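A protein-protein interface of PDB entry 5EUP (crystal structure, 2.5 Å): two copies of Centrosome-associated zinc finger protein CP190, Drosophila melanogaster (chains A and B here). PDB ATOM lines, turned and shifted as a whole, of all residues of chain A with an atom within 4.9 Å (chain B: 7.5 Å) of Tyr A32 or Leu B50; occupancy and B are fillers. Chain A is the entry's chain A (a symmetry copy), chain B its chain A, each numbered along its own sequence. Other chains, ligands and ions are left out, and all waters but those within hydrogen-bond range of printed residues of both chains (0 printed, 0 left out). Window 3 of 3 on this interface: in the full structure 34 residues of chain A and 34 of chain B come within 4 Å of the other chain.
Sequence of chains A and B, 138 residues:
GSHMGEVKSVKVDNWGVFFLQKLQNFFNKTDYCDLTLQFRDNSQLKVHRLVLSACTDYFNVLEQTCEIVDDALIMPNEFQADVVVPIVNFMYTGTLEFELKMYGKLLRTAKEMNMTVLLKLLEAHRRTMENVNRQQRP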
ATOM      1  N   LEU A  23       2.250  19.196  -1.535  1.00  0.00           N
ATOM      2  CA  LEU A  23       1.288  19.095  -0.439  1.00  0.00           C
ATOM      3  C   LEU A  23      -0.155  19.030  -0.937  1.00  0.00           C
ATOM      4  O   LEU A  23      -1.022  18.464  -0.271  1.00  0.00           O
ATOM      5  CB  LEU A  23       1.457  20.258   0.541  1.00  0.00           C
ATOM      6  CG  LEU A  23       2.751  20.259   1.355  1.00  0.00           C
ATOM      7  CD1 LEU A  23       2.748  21.391   2.369  1.00  0.00           C
ATOM      8  CD2 LEU A  23       2.954  18.917   2.043  1.00  0.00           C
ATOM      9  N   PHE A  26      -0.905  15.437  -1.796  1.00  0.00           N
ATOM     10  CA  PHE A  26      -1.121  14.681  -0.565  1.00  0.00           C
ATOM     11  C   PHE A  26      -2.527  14.945  -0.042  1.00  0.00           C
ATOM     12  O   PHE A  26      -3.188  14.043   0.477  1.00  0.00           O
ATOM     13  CB  PHE A  26      -0.087  15.076   0.493  1.00  0.00           C
ATOM     14  CG  PHE A  26       1.269  14.448   0.295  1.00  0.00           C
ATOM     15  CD1 PHE A  26       1.830  14.349  -0.968  1.00  0.00           C
ATOM     16  CD2 PHE A  26       1.992  13.978   1.379  1.00  0.00           C
ATOM     17  CE1 PHE A  26       3.077  13.780  -1.147  1.00  0.00           C
ATOM     18  CE2 PHE A  26       3.239  13.410   1.206  1.00  0.00           C
ATOM     19  CZ  PHE A  26       3.782  13.310  -0.059  1.00  0.00           C
ATOM     20  N   THR A  30      -5.548  12.174   0.400  1.00  0.00           N
ATOM     21  CA  THR A  30      -5.733  12.010   1.845  1.00  0.00           C
ATOM     22  C   THR A  30      -4.512  11.393   2.528  1.00  0.00           C
ATOM     23  O   THR A  30      -4.630  10.763   3.577  1.00  0.00           O
ATOM     24  CB  THR A  30      -6.994  11.175   2.184  1.00  0.00           C
ATOM     25  OG1 THR A  30      -6.796   9.812   1.785  1.00  0.00           O
ATOM     26  CG2 THR A  30      -8.215  11.741   1.476  1.00  0.00           C
ATOM     27  N   ASP A  31      -3.342  11.584   1.925  1.00  0.00           N
ATOM     28  CA  ASP A  31      -2.100  11.059   2.475  1.00  0.00           C
ATOM     29  C   ASP A  31      -1.638  11.863   3.686  1.00  0.00           C
ATOM     30  O   ASP A  31      -1.512  13.089   3.620  1.00  0.00           O
ATOM     31  CB  ASP A  31      -1.003  11.032   1.409  1.00  0.00           C
ATOM     32  CG  ASP A  31      -1.181   9.898   0.418  1.00  0.00           C
ATOM     33  OD1 ASP A  31      -1.742   8.851   0.805  1.00  0.00           O
ATOM     34  OD2 ASP A  31      -0.756  10.048  -0.749  1.00  0.00           O
ATOM     35  N   TYR A  32      -1.397  11.158   4.789  1.00  0.00           N
ATOM     36  CA  TYR A  32      -0.909  11.753   6.034  1.00  0.00           C
ATOM     37  C   TYR A  32      -1.825  12.848   6.585  1.00  0.00           C
ATOM     38  O   TYR A  32      -1.357  13.799   7.210  1.00  0.00           O
ATOM     39  CB  TYR A  32       0.513  12.296   5.858  1.00  0.00           C
ATOM     40  CG  TYR A  32       1.470  11.339   5.184  1.00  0.00           C
ATOM     41  CD1 TYR A  32       2.031  10.276   5.882  1.00  0.00           C
ATOM     42  CD2 TYR A  32       1.822  11.505   3.852  1.00  0.00           C
ATOM     43  CE1 TYR A  32       2.911   9.401   5.267  1.00  0.00           C
ATOM     44  CE2 TYR A  32       2.700  10.637   3.228  1.00  0.00           C
ATOM     45  CZ  TYR A  32       3.242   9.587   3.940  1.00  0.00           C
ATOM     46  OH  TYR A  32       4.116   8.724   3.320  1.00  0.00           O
ATOM     47  N   CYS A  33      -3.128  12.712   6.355  1.00  0.00           N
ATOM     48  CA  CYS A  33      -4.092  13.669   6.891  1.00  0.00           C
ATOM     49  C   CYS A  33      -4.454  13.336   8.335  1.00  0.00           C
ATOM     50  O   CYS A  33      -5.209  12.400   8.600  1.00  0.00           O
ATOM     51  CB  CYS A  33      -5.347  13.726   6.020  1.00  0.00           C
ATOM     52  SG  CYS A  33      -5.096  14.520   4.415  1.00  0.00           S
ATOM     53  N   ASP A  34      -3.908  14.114   9.263  1.00  0.00           N
ATOM     54  CA  ASP A  34      -4.088  13.866  10.690  1.00  0.00           C
ATOM     55  C   ASP A  34      -5.385  14.460  11.236  1.00  0.00           C
ATOM     56  O   ASP A  34      -5.948  13.953  12.208  1.00  0.00           O
ATOM     57  CB  ASP A  34      -2.890  14.408  11.476  1.00  0.00           C
ATOM     58  CG  ASP A  34      -2.477  15.799  11.027  1.00  0.00           C
ATOM     59  OD1 ASP A  34      -3.316  16.509  10.433  1.00  0.00           O
ATOM     60  OD2 ASP A  34      -1.314  16.184  11.269  1.00  0.00           O
ATOM     61  N   HIS A  48      -4.335  18.550   6.476  1.00  0.00           N
ATOM     62  CA  HIS A  48      -3.086  18.504   7.226  1.00  0.00           C
ATOM     63  C   HIS A  48      -3.087  19.589   8.293  1.00  0.00           C
ATOM     64  O   HIS A  48      -3.314  20.762   7.996  1.00  0.00           O
ATOM     65  CB  HIS A  48      -1.892  18.695   6.290  1.00  0.00           C
ATOM     66  CG  HIS A  48      -1.795  17.660   5.215  1.00  0.00           C
ATOM     67  ND1 HIS A  48      -1.596  17.981   3.889  1.00  0.00           N
ATOM     68  CD2 HIS A  48      -1.868  16.308   5.269  1.00  0.00           C
ATOM     69  CE1 HIS A  48      -1.552  16.873   3.173  1.00  0.00           C
ATOM     70  NE2 HIS A  48      -1.714  15.843   3.985  1.00  0.00           N
ATOM     71  N   LEU A  50      -0.699  20.866   9.879  1.00  0.00           N
ATOM     72  CA  LEU A  50       0.402  21.808   9.697  1.00  0.00           C
ATOM     73  C   LEU A  50       0.041  22.924   8.723  1.00  0.00           C
ATOM     74  O   LEU A  50       0.297  24.098   8.990  1.00  0.00           O
ATOM     75  CB  LEU A  50       1.657  21.083   9.206  1.00  0.00           C
ATOM     76  CG  LEU A  50       2.270  20.060  10.162  1.00  0.00           C
ATOM     77  CD1 LEU A  50       3.589  19.538   9.616  1.00  0.00           C
ATOM     78  CD2 LEU A  50       2.461  20.673  11.535  1.00  0.00           C
ATOM     79  N   LEU B  23       6.472  27.699   7.284  1.00  0.00           N
ATOM     80  CA  LEU B  23       6.941  26.403   7.770  1.00  0.00           C
ATOM     81  C   LEU B  23       8.381  26.461   8.278  1.00  0.00           C
ATOM     82  O   LEU B  23       8.773  25.676   9.142  1.00  0.00           O
ATOM     83  CB  LEU B  23       6.805  25.333   6.684  1.00  0.00           C
ATOM     84  CG  LEU B  23       5.375  24.946   6.308  1.00  0.00           C
ATOM     85  CD1 LEU B  23       5.372  23.799   5.311  1.00  0.00           C
ATOM     86  CD2 LEU B  23       4.572  24.586   7.550  1.00  0.00           C
ATOM     87  N   ASP B  34       6.924  16.595  14.824  1.00  0.00           N
ATOM     88  CA  ASP B  34       6.540  15.242  15.211  1.00  0.00           C
ATOM     89  C   ASP B  34       7.696  14.247  15.119  1.00  0.00           C
ATOM     90  O   ASP B  34       7.730  13.254  15.846  1.00  0.00           O
ATOM     91  CB  ASP B  34       5.364  14.761  14.355  1.00  0.00           C
ATOM     92  CG  ASP B  34       5.550  15.068  12.879  1.00  0.00           C
ATOM     93  OD1 ASP B  34       6.706  15.262  12.450  1.00  0.00           O
ATOM     94  OD2 ASP B  34       4.539  15.117  12.148  1.00  0.00           O
ATOM     95  N   LEU B  35       8.640  14.517  14.224  1.00  0.00           N
ATOM     96  CA  LEU B  35       9.770  13.618  14.016  1.00  0.00           C
ATOM     97  C   LEU B  35      11.055  14.163  14.629  1.00  0.00           C
ATOM     98  O   LEU B  35      11.453  15.297  14.361  1.00  0.00           O
ATOM     99  CB  LEU B  35       9.970  13.344  12.523  1.00  0.00           C
ATOM    100  CG  LEU B  35      11.116  12.400  12.153  1.00  0.00           C
ATOM    101  CD1 LEU B  35      10.948  11.051  12.835  1.00  0.00           C
ATOM    102  CD2 LEU B  35      11.202  12.235  10.644  1.00  0.00           C
ATOM    103  N   VAL B  47      12.087  17.985  13.224  1.00  0.00           N
ATOM    104  CA  VAL B  47      11.588  18.284  11.884  1.00  0.00           C
ATOM    105  C   VAL B  47      10.108  17.943  11.735  1.00  0.00           C
ATOM    106  O   VAL B  47       9.507  17.335  12.620  1.00  0.00           O
ATOM    107  CB  VAL B  47      12.373  17.517  10.799  1.00  0.00           C
ATOM    108  CG1 VAL B  47      13.824  17.973  10.760  1.00  0.00           C
ATOM    109  CG2 VAL B  47      12.279  16.017  11.036  1.00  0.00           C
ATOM    110  N   HIS B  48       9.531  18.342  10.606  1.00  0.00           N
ATOM    111  CA  HIS B  48       8.148  18.010  10.284  1.00  0.00           C
ATOM    112  C   HIS B  48       8.113  16.821   9.335  1.00  0.00           C
ATOM    113  O   HIS B  48       8.759  16.835   8.286  1.00  0.00           O
ATOM    114  CB  HIS B  48       7.444  19.207   9.647  1.00  0.00           C
ATOM    115  CG  HIS B  48       7.411  20.422  10.518  1.00  0.00           C
ATOM    116  ND1 HIS B  48       7.765  21.674  10.062  1.00  0.00           N
ATOM    117  CD2 HIS B  48       7.062  20.580  11.818  1.00  0.00           C
ATOM    118  CE1 HIS B  48       7.640  22.549  11.043  1.00  0.00           C
ATOM    119  NE2 HIS B  48       7.214  21.912  12.119  1.00  0.00           N
ATOM    120  N   ARG B  49       7.355  15.794   9.704  1.00  0.00           N
ATOM    121  CA  ARG B  49       7.296  14.566   8.919  1.00  0.00           C
ATOM    122  C   ARG B  49       6.674  14.799   7.544  1.00  0.00           C
ATOM    123  O   ARG B  49       6.972  14.079   6.593  1.00  0.00           O
ATOM    124  CB  ARG B  49       6.525  13.483   9.678  1.00  0.00           C
ATOM    125  CG  ARG B  49       6.752  12.077   9.153  1.00  0.00           C
ATOM    126  CD  ARG B  49       6.285  11.036  10.153  1.00  0.00           C
ATOM    127  NE  ARG B  49       6.827  11.288  11.486  1.00  0.00           N
ATOM    128  CZ  ARG B  49       6.778  10.418  12.490  1.00  0.00           C
ATOM    129  NH1 ARG B  49       6.221   9.228  12.314  1.00  0.00           N
ATOM    130  NH2 ARG B  49       7.296  10.735  13.670  1.00  0.00           N
ATOM    131  N   LEU B  50       5.819  15.811   7.446  1.00  0.00           N
ATOM    132  CA  LEU B  50       5.168  16.146   6.182  1.00  0.00           C
ATOM    133  C   LEU B  50       6.142  16.767   5.187  1.00  0.00           C
ATOM    134  O   LEU B  50       6.168  16.393   4.014  1.00  0.00           O
ATOM    135  CB  LEU B  50       3.993  17.098   6.415  1.00  0.00           C
ATOM    136  CG  LEU B  50       2.827  16.551   7.238  1.00  0.00           C
ATOM    137  CD1 LEU B  50       1.672  17.540   7.256  1.00  0.00           C
ATOM    138  CD2 LEU B  50       2.379  15.211   6.689  1.00  0.00           C
ATOM    139  N   VAL B  51       6.936  17.721   5.664  1.00  0.00           N
ATOM    140  CA  VAL B  51       7.885  18.438   4.820  1.00  0.00           C
ATOM    141  C   VAL B  51       8.911  17.494   4.201  1.00  0.00           C
ATOM    142  O   VAL B  51       9.224  17.591   3.015  1.00  0.00           O
ATOM    143  CB  VAL B  51       8.614  19.544   5.610  1.00  0.00           C
ATOM    144  CG1 VAL B  51       9.621  20.261   4.724  1.00  0.00           C
ATOM    145  CG2 VAL B  51       7.610  20.531   6.188  1.00  0.00           C
ATOM    146  N   LEU B  52       9.424  16.574   5.011  1.00  0.00           N
ATOM    147  CA  LEU B  52      10.420  15.614   4.549  1.00  0.00           C
ATOM    148  C   LEU B  52       9.825  14.613   3.561  1.00  0.00           C
ATOM    149  O   LEU B  52      10.435  14.303   2.537  1.00  0.00           O
ATOM    150  CB  LEU B  52      11.052  14.877   5.735  1.00  0.00           C
ATOM    151  CG  LEU B  52      12.267  15.516   6.416  1.00  0.00           C
ATOM    152  CD1 LEU B  52      11.964  16.916   6.932  1.00  0.00           C
ATOM    153  CD2 LEU B  52      12.762  14.630   7.548  1.00  0.00           C
ATOM    154  N   SER B  53       8.631  14.117   3.870  1.00  0.00           N
ATOM    155  CA  SER B  53       7.957  13.138   3.021  1.00  0.00           C
ATOM    156  C   SER B  53       7.573  13.726   1.666  1.00  0.00           C
ATOM    157  O   SER B  53       7.418  12.997   0.685  1.00  0.00           O
ATOM    158  CB  SER B  53       6.714  12.582   3.720  1.00  0.00           C
ATOM    159  OG  SER B  53       7.058  11.920   4.923  1.00  0.00           O
ATOM    160  N   ALA B  54       7.421  15.045   1.617  1.00  0.00           N
ATOM    161  CA  ALA B  54       7.054  15.730   0.385  1.00  0.00           C
ATOM    162  C   ALA B  54       8.260  15.922  -0.530  1.00  0.00           C
ATOM    163  O   ALA B  54       8.113  16.275  -1.700  1.00  0.00           O
ATOM    164  CB  ALA B  54       6.404  17.070   0.698  1.00  0.00           C
ATOM    165  N   CYS B  55       9.452  15.687   0.010  1.00  0.00           N
ATOM    166  CA  CYS B  55      10.683  15.878  -0.749  1.00  0.00           C
ATOM    167  C   CYS B  55      11.358  14.550  -1.082  1.00  0.00           C
ATOM    168  O   CYS B  55      12.074  14.440  -2.077  1.00  0.00           O
ATOM    169  CB  CYS B  55      11.647  16.781   0.022  1.00  0.00           C
ATOM    170  SG  CYS B  55      10.985  18.420   0.403  1.00  0.00           S
ATOM    171  N   THR B  56      11.123  13.545  -0.243  1.00  0.00           N
ATOM    172  CA  THR B  56      11.715  12.227  -0.439  1.00  0.00           C
ATOM    173  C   THR B  56      10.982  11.171   0.381  1.00  0.00           C
ATOM    174  O   THR B  56      10.209  11.497   1.283  1.00  0.00           O
ATOM    175  CB  THR B  56      13.204  12.217  -0.045  1.00  0.00           C
ATOM    176  OG1 THR B  56      13.773  10.935  -0.341  1.00  0.00           O
ATOM    177  CG2 THR B  56      13.361  12.507   1.440  1.00  0.00           C
ATOM    178  N   ASP B  57      11.226   9.904   0.061  1.00  0.00           N
ATOM    179  CA  ASP B  57      10.646   8.799   0.817  1.00  0.00           C
ATOM    180  C   ASP B  57      11.696   8.135   1.701  1.00  0.00           C
ATOM    181  O   ASP B  57      11.406   7.158   2.391  1.00  0.00           O
ATOM    182  CB  ASP B  57      10.029   7.763  -0.125  1.00  0.00           C
ATOM    183  CG  ASP B  57       8.839   8.306  -0.892  1.00  0.00           C
ATOM    184  OD1 ASP B  57       7.743   8.393  -0.301  1.00  0.00           O
ATOM    185  OD2 ASP B  57       8.999   8.636  -2.086  1.00  0.00           O
ATOM    186  N   ASN B  60      10.938   7.947   5.339  1.00  0.00           N
ATOM    187  CA  ASN B  60       9.860   6.993   5.566  1.00  0.00           C
ATOM    188  C   ASN B  60      10.396   5.568   5.642  1.00  0.00           C
ATOM    189  O   ASN B  60       9.815   4.708   6.305  1.00  0.00           O
ATOM    190  CB  ASN B  60       8.801   7.100   4.467  1.00  0.00           C
ATOM    191  CG  ASN B  60       8.088   8.438   4.473  1.00  0.00           C
ATOM    192  OD1 ASN B  60       7.985   9.096   5.509  1.00  0.00           O
ATOM    193  ND2 ASN B  60       7.588   8.846   3.313  1.00  0.00           N
ATOM    194  N   GLU B  63      12.077   4.951   9.136  1.00  0.00           N
ATOM    195  CA  GLU B  63      11.109   4.732  10.205  1.00  0.00           C
ATOM    196  C   GLU B  63      10.640   3.280  10.272  1.00  0.00           C
ATOM    197  O   GLU B  63      10.144   2.827  11.303  1.00  0.00           O
ATOM    198  CB  GLU B  63       9.911   5.668  10.037  1.00  0.00           C
ATOM    199  CG  GLU B  63      10.255   7.137  10.221  1.00  0.00           C
ATOM    200  CD  GLU B  63       9.127   8.057   9.807  1.00  0.00           C
ATOM    201  OE1 GLU B  63       8.560   8.736  10.688  1.00  0.00           O
ATOM    202  OE2 GLU B  63       8.808   8.106   8.600  1.00  0.00           O
ATOM    203  N   TYR B  92      13.226  23.271   3.410  1.00  0.00           N
ATOM    204  CA  TYR B  92      12.455  24.369   3.986  1.00  0.00           C
ATOM    205  C   TYR B  92      12.676  25.703   3.275  1.00  0.00           C
ATOM    206  O   TYR B  92      11.914  26.647   3.474  1.00  0.00           O
ATOM    207  CB  TYR B  92      12.772  24.523   5.478  1.00  0.00           C
ATOM    208  CG  TYR B  92      12.120  23.483   6.361  1.00  0.00           C
ATOM    209  CD1 TYR B  92      10.811  23.640   6.799  1.00  0.00           C
ATOM    210  CD2 TYR B  92      12.814  22.349   6.764  1.00  0.00           C
ATOM    211  CE1 TYR B  92      10.209  22.695   7.609  1.00  0.00           C
ATOM    212  CE2 TYR B  92      12.221  21.397   7.573  1.00  0.00           C
ATOM    213  CZ  TYR B  92      10.918  21.576   7.992  1.00  0.00           C
ATOM    214  OH  TYR B  92      10.320  20.634   8.797  1.00  0.00           O
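O of Ser B53 touches CZ of Phe A26, 3.7 Å away. CD2 of Leu B50 touches CB of Tyr A32, 3.6 Å away. His A48 touches Leu B50. CB of His B48 touches CD1 of Leu A50, at 3.9 Å. CD1 of Leu A50 touches CD1 of Leu B50, at 3.6 Å.
OG of Ser B53 is in hydrogen-bond range of O of Arg B49. The side-chain hydroxyl of Ser B53 lies within hydrogen-bond range of the side-chain amide oxygen of Asn B60 (3.0 Å). The side-chain sulfur (SG) of Cys A33 sits at hydrogen-bond distance from a ring nitrogen (NE2) of His A48 (3.7 Å). The backbone carbonyl oxygen of Phe A26 sits at hydrogen-bond distance from the backbone NH of Asp A31. O of Asp A31 lies within hydrogen-bond range of NE2 of His A48 (2.8 Å). The backbone NH (N) of His B48 lies within hydrogen-bond range of the side-chain hydroxyl (OH) of Tyr B92 (3.0 Å).
His A48 touches Leu B50, and with the chains exchanged Leu A50 touches His B48. Leu A50 touches its own counterpart, Leu B50. Positions printed for both chains: 23, 34, 48 and 50. Of the 6 pairs that touch across the chains among the printed residues, 3 have their exchanged pair printed and touching as well.
Tyr A32 touches just these residues of chain B: Leu B50 and Asn B60. Of chain A, only Tyr A32, His A48 and Leu A50 come within 4 Å of Leu B50. Printed residues of chain B within 4 Å of His A48: Leu B50 (3.9 Å). Of the printed residues of chain A, His B48 touches Leu A50. Printed residues of chain B within 4 Å of Leu A50: His B48 (3.9 Å) and Leu B50 (3.6 Å). Printed residues of chain A within 4 Å of Asn B60: Tyr A32. The nearest residue of chain B that does not touch Tyr A32 is Ser B53 (4.5 Å).
Of the 9 printed residues of chain A, 4 touch a printed residue of chain B. Hydrophobic or aromatic side chains of chain A that line the printed part of chain B: Phe A26, Tyr A32, His A48 and Leu A50. Printed residues of chain B that touch a printed residue of chain A: His B48, Leu B50, Ser B53 and Asn B60. Among the printed residues, no Asp or Glu carboxylate lies within 4 Å of a Lys or Arg side-chain nitrogen of the other chain.
OH of Tyr A32 is in hydrogen-bond range of ND2 of Asn B60, at 3.5 Å.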
